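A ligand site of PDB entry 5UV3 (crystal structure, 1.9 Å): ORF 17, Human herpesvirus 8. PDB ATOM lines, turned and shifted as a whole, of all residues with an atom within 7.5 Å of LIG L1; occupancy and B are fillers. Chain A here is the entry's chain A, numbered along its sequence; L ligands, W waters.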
ATOM      1  N   PHE A  73      -2.209  -6.386 -16.604  1.00  0.00           N
ATOM      2  CA  PHE A  73      -2.412  -6.870 -15.248  1.00  0.00           C
ATOM      3  C   PHE A  73      -3.363  -8.078 -15.216  1.00  0.00           C
ATOM      4  O   PHE A  73      -3.105  -9.058 -14.489  1.00  0.00           O
ATOM      5  CB  PHE A  73      -2.927  -5.760 -14.345  1.00  0.00           C
ATOM      6  CG  PHE A  73      -3.223  -6.216 -12.947  1.00  0.00           C
ATOM      7  CD1 PHE A  73      -2.202  -6.384 -12.046  1.00  0.00           C
ATOM      8  CD2 PHE A  73      -4.527  -6.490 -12.543  1.00  0.00           C
ATOM      9  CE1 PHE A  73      -2.451  -6.780 -10.728  1.00  0.00           C
ATOM     10  CE2 PHE A  73      -4.803  -6.933 -11.233  1.00  0.00           C
ATOM     11  CZ  PHE A  73      -3.764  -7.063 -10.331  1.00  0.00           C
ATOM     12  N   LEU A  76      -1.564 -11.161 -16.493  1.00  0.00           N
ATOM     13  CA  LEU A  76      -0.546 -11.653 -15.572  1.00  0.00           C
ATOM     14  C   LEU A  76      -1.184 -12.312 -14.351  1.00  0.00           C
ATOM     15  O   LEU A  76      -0.850 -13.449 -13.994  1.00  0.00           O
ATOM     16  CB  LEU A  76       0.373 -10.531 -15.143  1.00  0.00           C
ATOM     17  CG  LEU A  76       1.463 -10.865 -14.119  1.00  0.00           C
ATOM     18  CD1 LEU A  76       2.462 -11.940 -14.653  1.00  0.00           C
ATOM     19  CD2 LEU A  76       2.162  -9.562 -13.766  1.00  0.00           C
ATOM     20  N   ALA A  77      -2.114 -11.604 -13.703  1.00  0.00           N
ATOM     21  CA  ALA A  77      -2.782 -12.146 -12.534  1.00  0.00           C
ATOM     22  C   ALA A  77      -3.452 -13.484 -12.850  1.00  0.00           C
ATOM     23  O   ALA A  77      -3.393 -14.446 -12.064  1.00  0.00           O
ATOM     24  CB  ALA A  77      -3.830 -11.144 -12.036  1.00  0.00           C
ATOM     25  N   ARG A  79      -2.794 -15.633 -15.322  1.00  0.00           N
ATOM     26  CA  ARG A  79      -1.769 -16.641 -15.517  1.00  0.00           C
ATOM     27  C   ARG A  79      -1.211 -17.148 -14.183  1.00  0.00           C
ATOM     28  O   ARG A  79      -1.025 -18.360 -13.979  1.00  0.00           O
ATOM     29  CB  ARG A  79      -0.630 -16.109 -16.390  1.00  0.00           C
ATOM     30  CG  ARG A  79       0.450 -17.168 -16.682  1.00  0.00           C
ATOM     31  CD  ARG A  79       1.540 -16.693 -17.681  1.00  0.00           C
ATOM     32  NE  ARG A  79       2.367 -15.639 -17.118  1.00  0.00           N
ATOM     33  CZ  ARG A  79       3.513 -15.836 -16.462  1.00  0.00           C
ATOM     34  NH1 ARG A  79       3.968 -17.064 -16.325  1.00  0.00           N
ATOM     35  NH2 ARG A  79       4.192 -14.812 -15.977  1.00  0.00           N
ATOM     36  N   LEU A  80      -0.941 -16.226 -13.254  1.00  0.00           N
ATOM     37  CA  LEU A  80      -0.488 -16.630 -11.929  1.00  0.00           C
ATOM     38  C   LEU A  80      -1.534 -17.504 -11.241  1.00  0.00           C
ATOM     39  O   LEU A  80      -1.187 -18.510 -10.583  1.00  0.00           O
ATOM     40  CB  LEU A  80      -0.198 -15.395 -11.043  1.00  0.00           C
ATOM     41  CG  LEU A  80       1.002 -14.620 -11.555  1.00  0.00           C
ATOM     42  CD1 LEU A  80       1.306 -13.284 -10.699  1.00  0.00           C
ATOM     43  CD2 LEU A  80       2.159 -15.508 -11.649  1.00  0.00           C
ATOM     44  N   ALA A  81      -2.792 -17.108 -11.328  1.00  0.00           N
ATOM     45  CA  ALA A  81      -3.841 -17.821 -10.622  1.00  0.00           C
ATOM     46  C   ALA A  81      -3.972 -19.267 -11.134  1.00  0.00           C
ATOM     47  O   ALA A  81      -4.381 -20.155 -10.376  1.00  0.00           O
ATOM     48  CB  ALA A  81      -5.150 -17.072 -10.784  1.00  0.00           C
ATOM     49  N   THR A  83      -1.256 -21.058 -12.625  1.00  0.00           N
ATOM     50  CA  THR A  83      -0.027 -21.842 -12.742  1.00  0.00           C
ATOM     51  C   THR A  83       0.945 -21.645 -11.609  1.00  0.00           C
ATOM     52  O   THR A  83       1.971 -22.313 -11.608  1.00  0.00           O
ATOM     53  CB  THR A  83       0.720 -21.502 -14.034  1.00  0.00           C
ATOM     54  OG1 THR A  83       1.131 -20.132 -13.937  1.00  0.00           O
ATOM     55  CG2 THR A  83      -0.213 -21.697 -15.264  1.00  0.00           C
ATOM     56  N   SER A  84       0.694 -20.718 -10.671  1.00  0.00           N
ATOM     57  CA  SER A  84       1.674 -20.395  -9.636  1.00  0.00           C
ATOM     58  C   SER A  84       1.288 -21.068  -8.330  1.00  0.00           C
ATOM     59  O   SER A  84       0.277 -20.692  -7.711  1.00  0.00           O
ATOM     60  CB  SER A  84       1.778 -18.878  -9.415  1.00  0.00           C
ATOM     61  OG  SER A  84       2.546 -18.671  -8.251  1.00  0.00           O
ATOM     62  N   HIS A  85       2.087 -22.058  -7.914  1.00  0.00           N
ATOM     63  CA  HIS A  85       1.823 -22.664  -6.602  1.00  0.00           C
ATOM     64  C   HIS A  85       1.951 -21.628  -5.470  1.00  0.00           C
ATOM     65  O   HIS A  85       1.186 -21.694  -4.505  1.00  0.00           O
ATOM     66  CB  HIS A  85       2.789 -23.843  -6.369  1.00  0.00           C
ATOM     67  N   VAL A  86       2.835 -20.648  -5.625  1.00  0.00           N
ATOM     68  CA  VAL A  86       3.003 -19.591  -4.589  1.00  0.00           C
ATOM     69  C   VAL A  86       1.751 -18.744  -4.480  1.00  0.00           C
ATOM     70  O   VAL A  86       1.259 -18.475  -3.371  1.00  0.00           O
ATOM     71  CB  VAL A  86       4.274 -18.747  -4.869  1.00  0.00           C
ATOM     72  CG1 VAL A  86       4.387 -17.599  -3.891  1.00  0.00           C
ATOM     73  CG2 VAL A  86       5.518 -19.618  -4.729  1.00  0.00           C
ATOM     74  N   ALA A  87       1.207 -18.301  -5.635  1.00  0.00           N
ATOM     75  CA  ALA A  87       0.006 -17.484  -5.612  1.00  0.00           C
ATOM     76  C   ALA A  87      -1.160 -18.232  -4.959  1.00  0.00           C
ATOM     77  O   ALA A  87      -1.956 -17.667  -4.200  1.00  0.00           O
ATOM     78  CB  ALA A  87      -0.350 -17.065  -7.039  1.00  0.00           C
ATOM     79  N   ARG A  88      -1.216 -19.542  -5.199  1.00  0.00           N
ATOM     80  CA  ARG A  88      -2.337 -20.323  -4.738  1.00  0.00           C
ATOM     81  C   ARG A  88      -2.166 -20.852  -3.327  1.00  0.00           C
ATOM     82  O   ARG A  88      -3.151 -21.304  -2.729  1.00  0.00           O
ATOM     83  CB  ARG A  88      -2.532 -21.513  -5.703  1.00  0.00           C
ATOM     84  CG  ARG A  88      -3.007 -21.064  -7.072  1.00  0.00           C
ATOM     85  CD  ARG A  88      -2.887 -22.184  -8.096  1.00  0.00           C
ATOM     86  NE  ARG A  88      -3.871 -23.241  -7.814  1.00  0.00           N
ATOM     87  CZ  ARG A  88      -5.047 -23.337  -8.410  1.00  0.00           C
ATOM     88  NH1 ARG A  88      -5.354 -22.488  -9.376  1.00  0.00           N
ATOM     89  NH2 ARG A  88      -5.859 -24.355  -8.095  1.00  0.00           N
ATOM     90  N   ILE A 102      -7.459 -15.270  -5.771  1.00  0.00           N
ATOM     91  CA  ILE A 102      -6.106 -14.749  -5.684  1.00  0.00           C
ATOM     92  C   ILE A 102      -6.156 -13.252  -5.354  1.00  0.00           C
ATOM     93  O   ILE A 102      -5.513 -12.777  -4.399  1.00  0.00           O
ATOM     94  CB  ILE A 102      -5.387 -15.049  -7.020  1.00  0.00           C
ATOM     95  CG1 ILE A 102      -5.018 -16.516  -7.098  1.00  0.00           C
ATOM     96  CG2 ILE A 102      -4.194 -14.093  -7.326  1.00  0.00           C
ATOM     97  CD1 ILE A 102      -4.120 -16.780  -6.062  1.00  0.00           C
ATOM     98  N   TRP A 106      -4.724 -11.729  -1.863  1.00  0.00           N
ATOM     99  CA  TRP A 106      -3.445 -11.004  -1.853  1.00  0.00           C
ATOM    100  C   TRP A 106      -3.606  -9.497  -1.803  1.00  0.00           C
ATOM    101  O   TRP A 106      -2.693  -8.810  -1.340  1.00  0.00           O
ATOM    102  CB  TRP A 106      -2.601 -11.384  -3.088  1.00  0.00           C
ATOM    103  CG  TRP A 106      -1.973 -12.798  -3.027  1.00  0.00           C
ATOM    104  CD1 TRP A 106      -2.541 -13.989  -3.458  1.00  0.00           C
ATOM    105  CD2 TRP A 106      -0.656 -13.144  -2.550  1.00  0.00           C
ATOM    106  NE1 TRP A 106      -1.655 -15.045  -3.278  1.00  0.00           N
ATOM    107  CE2 TRP A 106      -0.500 -14.551  -2.721  1.00  0.00           C
ATOM    108  CE3 TRP A 106       0.406 -12.406  -2.023  1.00  0.00           C
ATOM    109  CZ2 TRP A 106       0.665 -15.217  -2.344  1.00  0.00           C
ATOM    110  CZ3 TRP A 106       1.550 -13.059  -1.649  1.00  0.00           C
ATOM    111  CH2 TRP A 106       1.666 -14.464  -1.801  1.00  0.00           C
ATOM    112  N   PHE A 186      -0.391   0.315 -15.915  1.00  0.00           N
ATOM    113  CA  PHE A 186       0.333  -0.856 -15.376  1.00  0.00           C
ATOM    114  C   PHE A 186       1.158  -1.547 -16.439  1.00  0.00           C
ATOM    115  O   PHE A 186       0.657  -1.900 -17.515  1.00  0.00           O
ATOM    116  CB  PHE A 186      -0.642  -1.865 -14.756  1.00  0.00           C
ATOM    117  CG  PHE A 186       0.040  -3.130 -14.247  1.00  0.00           C
ATOM    118  CD1 PHE A 186       0.528  -3.184 -12.929  1.00  0.00           C
ATOM    119  CD2 PHE A 186       0.235  -4.208 -15.098  1.00  0.00           C
ATOM    120  CE1 PHE A 186       1.166  -4.363 -12.445  1.00  0.00           C
ATOM    121  CE2 PHE A 186       0.863  -5.406 -14.621  1.00  0.00           C
ATOM    122  CZ  PHE A 186       1.343  -5.458 -13.309  1.00  0.00           C
ATOM    123  N   SER A 188       3.821  -4.990 -16.526  1.00  0.00           N
ATOM    124  CA  SER A 188       4.279  -6.156 -15.764  1.00  0.00           C
ATOM    125  C   SER A 188       5.689  -5.909 -15.254  1.00  0.00           C
ATOM    126  O   SER A 188       6.589  -5.616 -16.068  1.00  0.00           O
ATOM    127  CB  SER A 188       4.239  -7.441 -16.603  1.00  0.00           C
ATOM    128  OG  SER A 188       4.845  -8.538 -15.917  1.00  0.00           O
ATOM    129  N   PRO A 189       5.933  -5.967 -13.937  1.00  0.00           N
ATOM    130  CA  PRO A 189       7.323  -5.827 -13.454  1.00  0.00           C
ATOM    131  C   PRO A 189       8.184  -7.067 -13.685  1.00  0.00           C
ATOM    132  O   PRO A 189       9.306  -7.132 -13.166  1.00  0.00           O
ATOM    133  CB  PRO A 189       7.139  -5.515 -11.963  1.00  0.00           C
ATOM    134  CG  PRO A 189       5.817  -6.117 -11.603  1.00  0.00           C
ATOM    135  CD  PRO A 189       4.963  -5.968 -12.830  1.00  0.00           C
ATOM    136  N   LEU A 190       7.688  -8.032 -14.485  1.00  0.00           N
ATOM    137  CA  LEU A 190       8.458  -9.211 -14.879  1.00  0.00           C
ATOM    138  C   LEU A 190       9.535  -8.944 -15.921  1.00  0.00           C
ATOM    139  O   LEU A 190      10.726  -9.103 -15.638  1.00  0.00           O
ATOM    140  CB  LEU A 190       7.568 -10.330 -15.425  1.00  0.00           C
ATOM    141  CG  LEU A 190       6.754 -11.138 -14.417  1.00  0.00           C
ATOM    142  CD1 LEU A 190       6.036 -12.297 -15.107  1.00  0.00           C
ATOM    143  CD2 LEU A 190       7.673 -11.637 -13.357  1.00  0.00           C
HETATM  144  C1  LIG L   1       9.475 -12.081  -5.073  1.00  0.00           C
HETATM  145  C2  LIG L   1       7.948 -14.426  -5.339  1.00  0.00           C
HETATM  146  C3  LIG L   1       5.627 -15.823  -9.791  1.00  0.00           C
HETATM  147  C4  LIG L   1       6.149 -16.804 -12.312  1.00  0.00           C
HETATM  148  C5  LIG L   1       5.051 -17.220 -11.613  1.00  0.00           C
HETATM  149  C6  LIG L   1       4.764 -16.731 -10.361  1.00  0.00           C
HETATM  150  C7  LIG L   1       8.557 -12.187  -9.915  1.00  0.00           C
HETATM  151  C8  LIG L   1       2.783 -14.083  -5.914  1.00  0.00           C
HETATM  152  C9  LIG L   1       2.859 -13.210  -4.831  1.00  0.00           C
HETATM  153  C10 LIG L   1       4.071 -12.598  -4.501  1.00  0.00           C
HETATM  154  C11 LIG L   1       5.226 -12.882  -5.250  1.00  0.00           C
HETATM  155  N1  LIG L   1       5.122 -13.733  -6.292  1.00  0.00           N
HETATM  156  C12 LIG L   1       3.952 -14.361  -6.615  1.00  0.00           C
HETATM  157  C13 LIG L   1       6.627 -12.306  -4.986  1.00  0.00           C
HETATM  158  C14 LIG L   1       7.501 -13.390  -4.343  1.00  0.00           C
HETATM  159  C15 LIG L   1       8.813 -12.776  -3.895  1.00  0.00           C
HETATM  160  C16 LIG L   1       9.927 -13.096  -6.105  1.00  0.00           C
HETATM  161  C17 LIG L   1       8.712 -13.882  -6.548  1.00  0.00           C
HETATM  162  C18 LIG L   1       4.042 -15.274  -7.833  1.00  0.00           C
HETATM  163  O1  LIG L   1       3.106 -15.980  -8.109  1.00  0.00           O
HETATM  164  N2  LIG L   1       5.294 -15.227  -8.540  1.00  0.00           N
HETATM  165  C19 LIG L   1       6.742 -15.347 -10.516  1.00  0.00           C
HETATM  166  C20 LIG L   1       7.025 -15.855 -11.783  1.00  0.00           C
HETATM  167  C21 LIG L   1       6.293 -17.422 -13.686  1.00  0.00           C
HETATM  168  O2  LIG L   1       6.892 -16.757 -14.582  1.00  0.00           O
HETATM  169  O3  LIG L   1       5.735 -18.524 -13.933  1.00  0.00           O
HETATM  170  N3  LIG L   1       7.645 -14.435  -9.915  1.00  0.00           N
HETATM  171  C22 LIG L   1       7.472 -13.038  -9.871  1.00  0.00           C
HETATM  172  C23 LIG L   1       8.353 -10.796  -9.883  1.00  0.00           C
HETATM  173  C24 LIG L   1       7.047 -10.273  -9.820  1.00  0.00           C
HETATM  174  C25 LIG L   1       5.966 -11.164  -9.772  1.00  0.00           C
HETATM  175  C26 LIG L   1       6.183 -12.546  -9.819  1.00  0.00           C
HETATM  176  O4  LIG L   1       4.617 -10.738  -9.690  1.00  0.00           O
HETATM  177  C27 LIG L   1       3.986 -10.908  -8.412  1.00  0.00           C
HETATM  178  F1  LIG L   1       4.778 -10.881  -7.314  1.00  0.00           F
HETATM  179  F2  LIG L   1       3.202  -9.859  -8.333  1.00  0.00           F
HETATM  180  F3  LIG L   1       3.249 -12.010  -8.354  1.00  0.00           F
HETATM  181  C1  LG2 L   2      -1.544 -10.562  -8.382  1.00  0.00           C
HETATM  182  C2  LG2 L   2      -0.289 -10.691  -5.728  1.00  0.00           C
HETATM  183  C3  LG2 L   2       6.231  -7.647  -6.454  1.00  0.00           C
HETATM  184  C4  LG2 L   2       8.553  -7.256  -7.968  1.00  0.00           C
HETATM  185  C5  LG2 L   2       8.435  -8.372  -7.153  1.00  0.00           C
HETATM  186  C6  LG2 L   2       7.267  -8.561  -6.401  1.00  0.00           C
HETATM  187  C7  LG2 L   2       3.457  -4.448  -8.106  1.00  0.00           C
HETATM  188  C8  LG2 L   2       3.115  -8.828  -2.625  1.00  0.00           C
HETATM  189  C9  LG2 L   2       1.763  -8.927  -2.353  1.00  0.00           C
HETATM  190  C10 LG2 L   2       0.740  -8.747  -3.282  1.00  0.00           C
HETATM  191  C11 LG2 L   2       1.114  -8.417  -4.576  1.00  0.00           C
HETATM  192  N1  LG2 L   2       2.444  -8.304  -4.866  1.00  0.00           N
HETATM  193  C12 LG2 L   2       3.442  -8.511  -3.944  1.00  0.00           C
HETATM  194  C13 LG2 L   2       0.055  -8.214  -5.649  1.00  0.00           C
HETATM  195  C14 LG2 L   2       0.026  -9.456  -6.557  1.00  0.00           C
HETATM  196  C15 LG2 L   2      -1.033  -9.292  -7.654  1.00  0.00           C
HETATM  197  C16 LG2 L   2      -1.286 -11.930  -7.734  1.00  0.00           C
HETATM  198  C17 LG2 L   2      -0.243 -11.900  -6.643  1.00  0.00           C
HETATM  199  C18 LG2 L   2       4.880  -8.368  -4.430  1.00  0.00           C
HETATM  200  O1  LG2 L   2       5.854  -8.658  -3.754  1.00  0.00           O
HETATM  201  N2  LG2 L   2       5.007  -7.849  -5.733  1.00  0.00           N
HETATM  202  C19 LG2 L   2       6.367  -6.571  -7.317  1.00  0.00           C
HETATM  203  C20 LG2 L   2       7.534  -6.342  -8.058  1.00  0.00           C
HETATM  204  C21 LG2 L   2       9.818  -7.062  -8.809  1.00  0.00           C
HETATM  205  O2  LG2 L   2      10.170  -5.912  -9.135  1.00  0.00           O
HETATM  206  O3  LG2 L   2      10.490  -8.063  -9.157  1.00  0.00           O
HETATM  207  N3  LG2 L   2       5.373  -5.612  -7.364  1.00  0.00           N
HETATM  208  C22 LG2 L   2       4.129  -5.660  -7.963  1.00  0.00           C
HETATM  209  C23 LG2 L   2       2.189  -4.506  -8.660  1.00  0.00           C
HETATM  210  C24 LG2 L   2       1.647  -5.751  -9.070  1.00  0.00           C
HETATM  211  C25 LG2 L   2       2.382  -6.902  -8.880  1.00  0.00           C
HETATM  212  C26 LG2 L   2       3.618  -6.871  -8.323  1.00  0.00           C
HETATM  213  O4  LG2 L   2       1.879  -8.176  -9.231  1.00  0.00           O
HETATM  214  C27 LG2 L   2       1.870  -8.576 -10.579  1.00  0.00           C
HETATM  215  F1  LG2 L   2       3.092  -8.343 -11.162  1.00  0.00           F
HETATM  216  F2  LG2 L   2       0.901  -7.848 -11.174  1.00  0.00           F
HETATM  217  F3  LG2 L   2       1.623  -9.929 -10.587  1.00  0.00           F
HETATM  218  O   HOH W   1       6.394 -20.369 -15.940  1.00  0.00           O
HETATM  219  O   HOH W   2       3.927 -19.654 -12.630  1.00  0.00           O
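The guanidinium group (NH1) of Arg 79 is in salt-bridge range of an oxygen (O3) of LIG L1. O1 of LIG L1 is in hydrogen-bond range of OG of Ser 84 (2.8 Å).
The side-chain hydroxyl (OG) of Ser 84 lies within hydrogen-bond range of the backbone NH (N) of Ala 87 (3.0 Å). The backbone carbonyl oxygen (O) of Arg 79 lies within hydrogen-bond range of the side-chain hydroxyl (OG1) of Thr 83. The side-chain hydroxyl (OG) of Ser 84 sits close to the backbone NH (N) of Val 86 (3.3 Å). The backbone carbonyl oxygen (O) of Ala 87 sits at hydrogen-bond distance from the indole nitrogen (NE1) of Trp 106 (2.8 Å). The side-chain hydroxyl (OG) of Ser 188 sits close to the backbone NH (N) of Leu 190 (3.2 Å).
Merely in contact with LIG L1: Leu 80, Trp 106, Leu 190 and Ala 87. Six residues have an atom within 4 Å of LIG L1: Arg 79, Leu 80, Ser 84, Ala 87, Trp 106 and Leu 190.
Water W2 bridges an oxygen (O3) of LIG L1 (2.5 Å) and the side-chain hydroxyl (OG1) of Thr 83 (3.1 Å).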
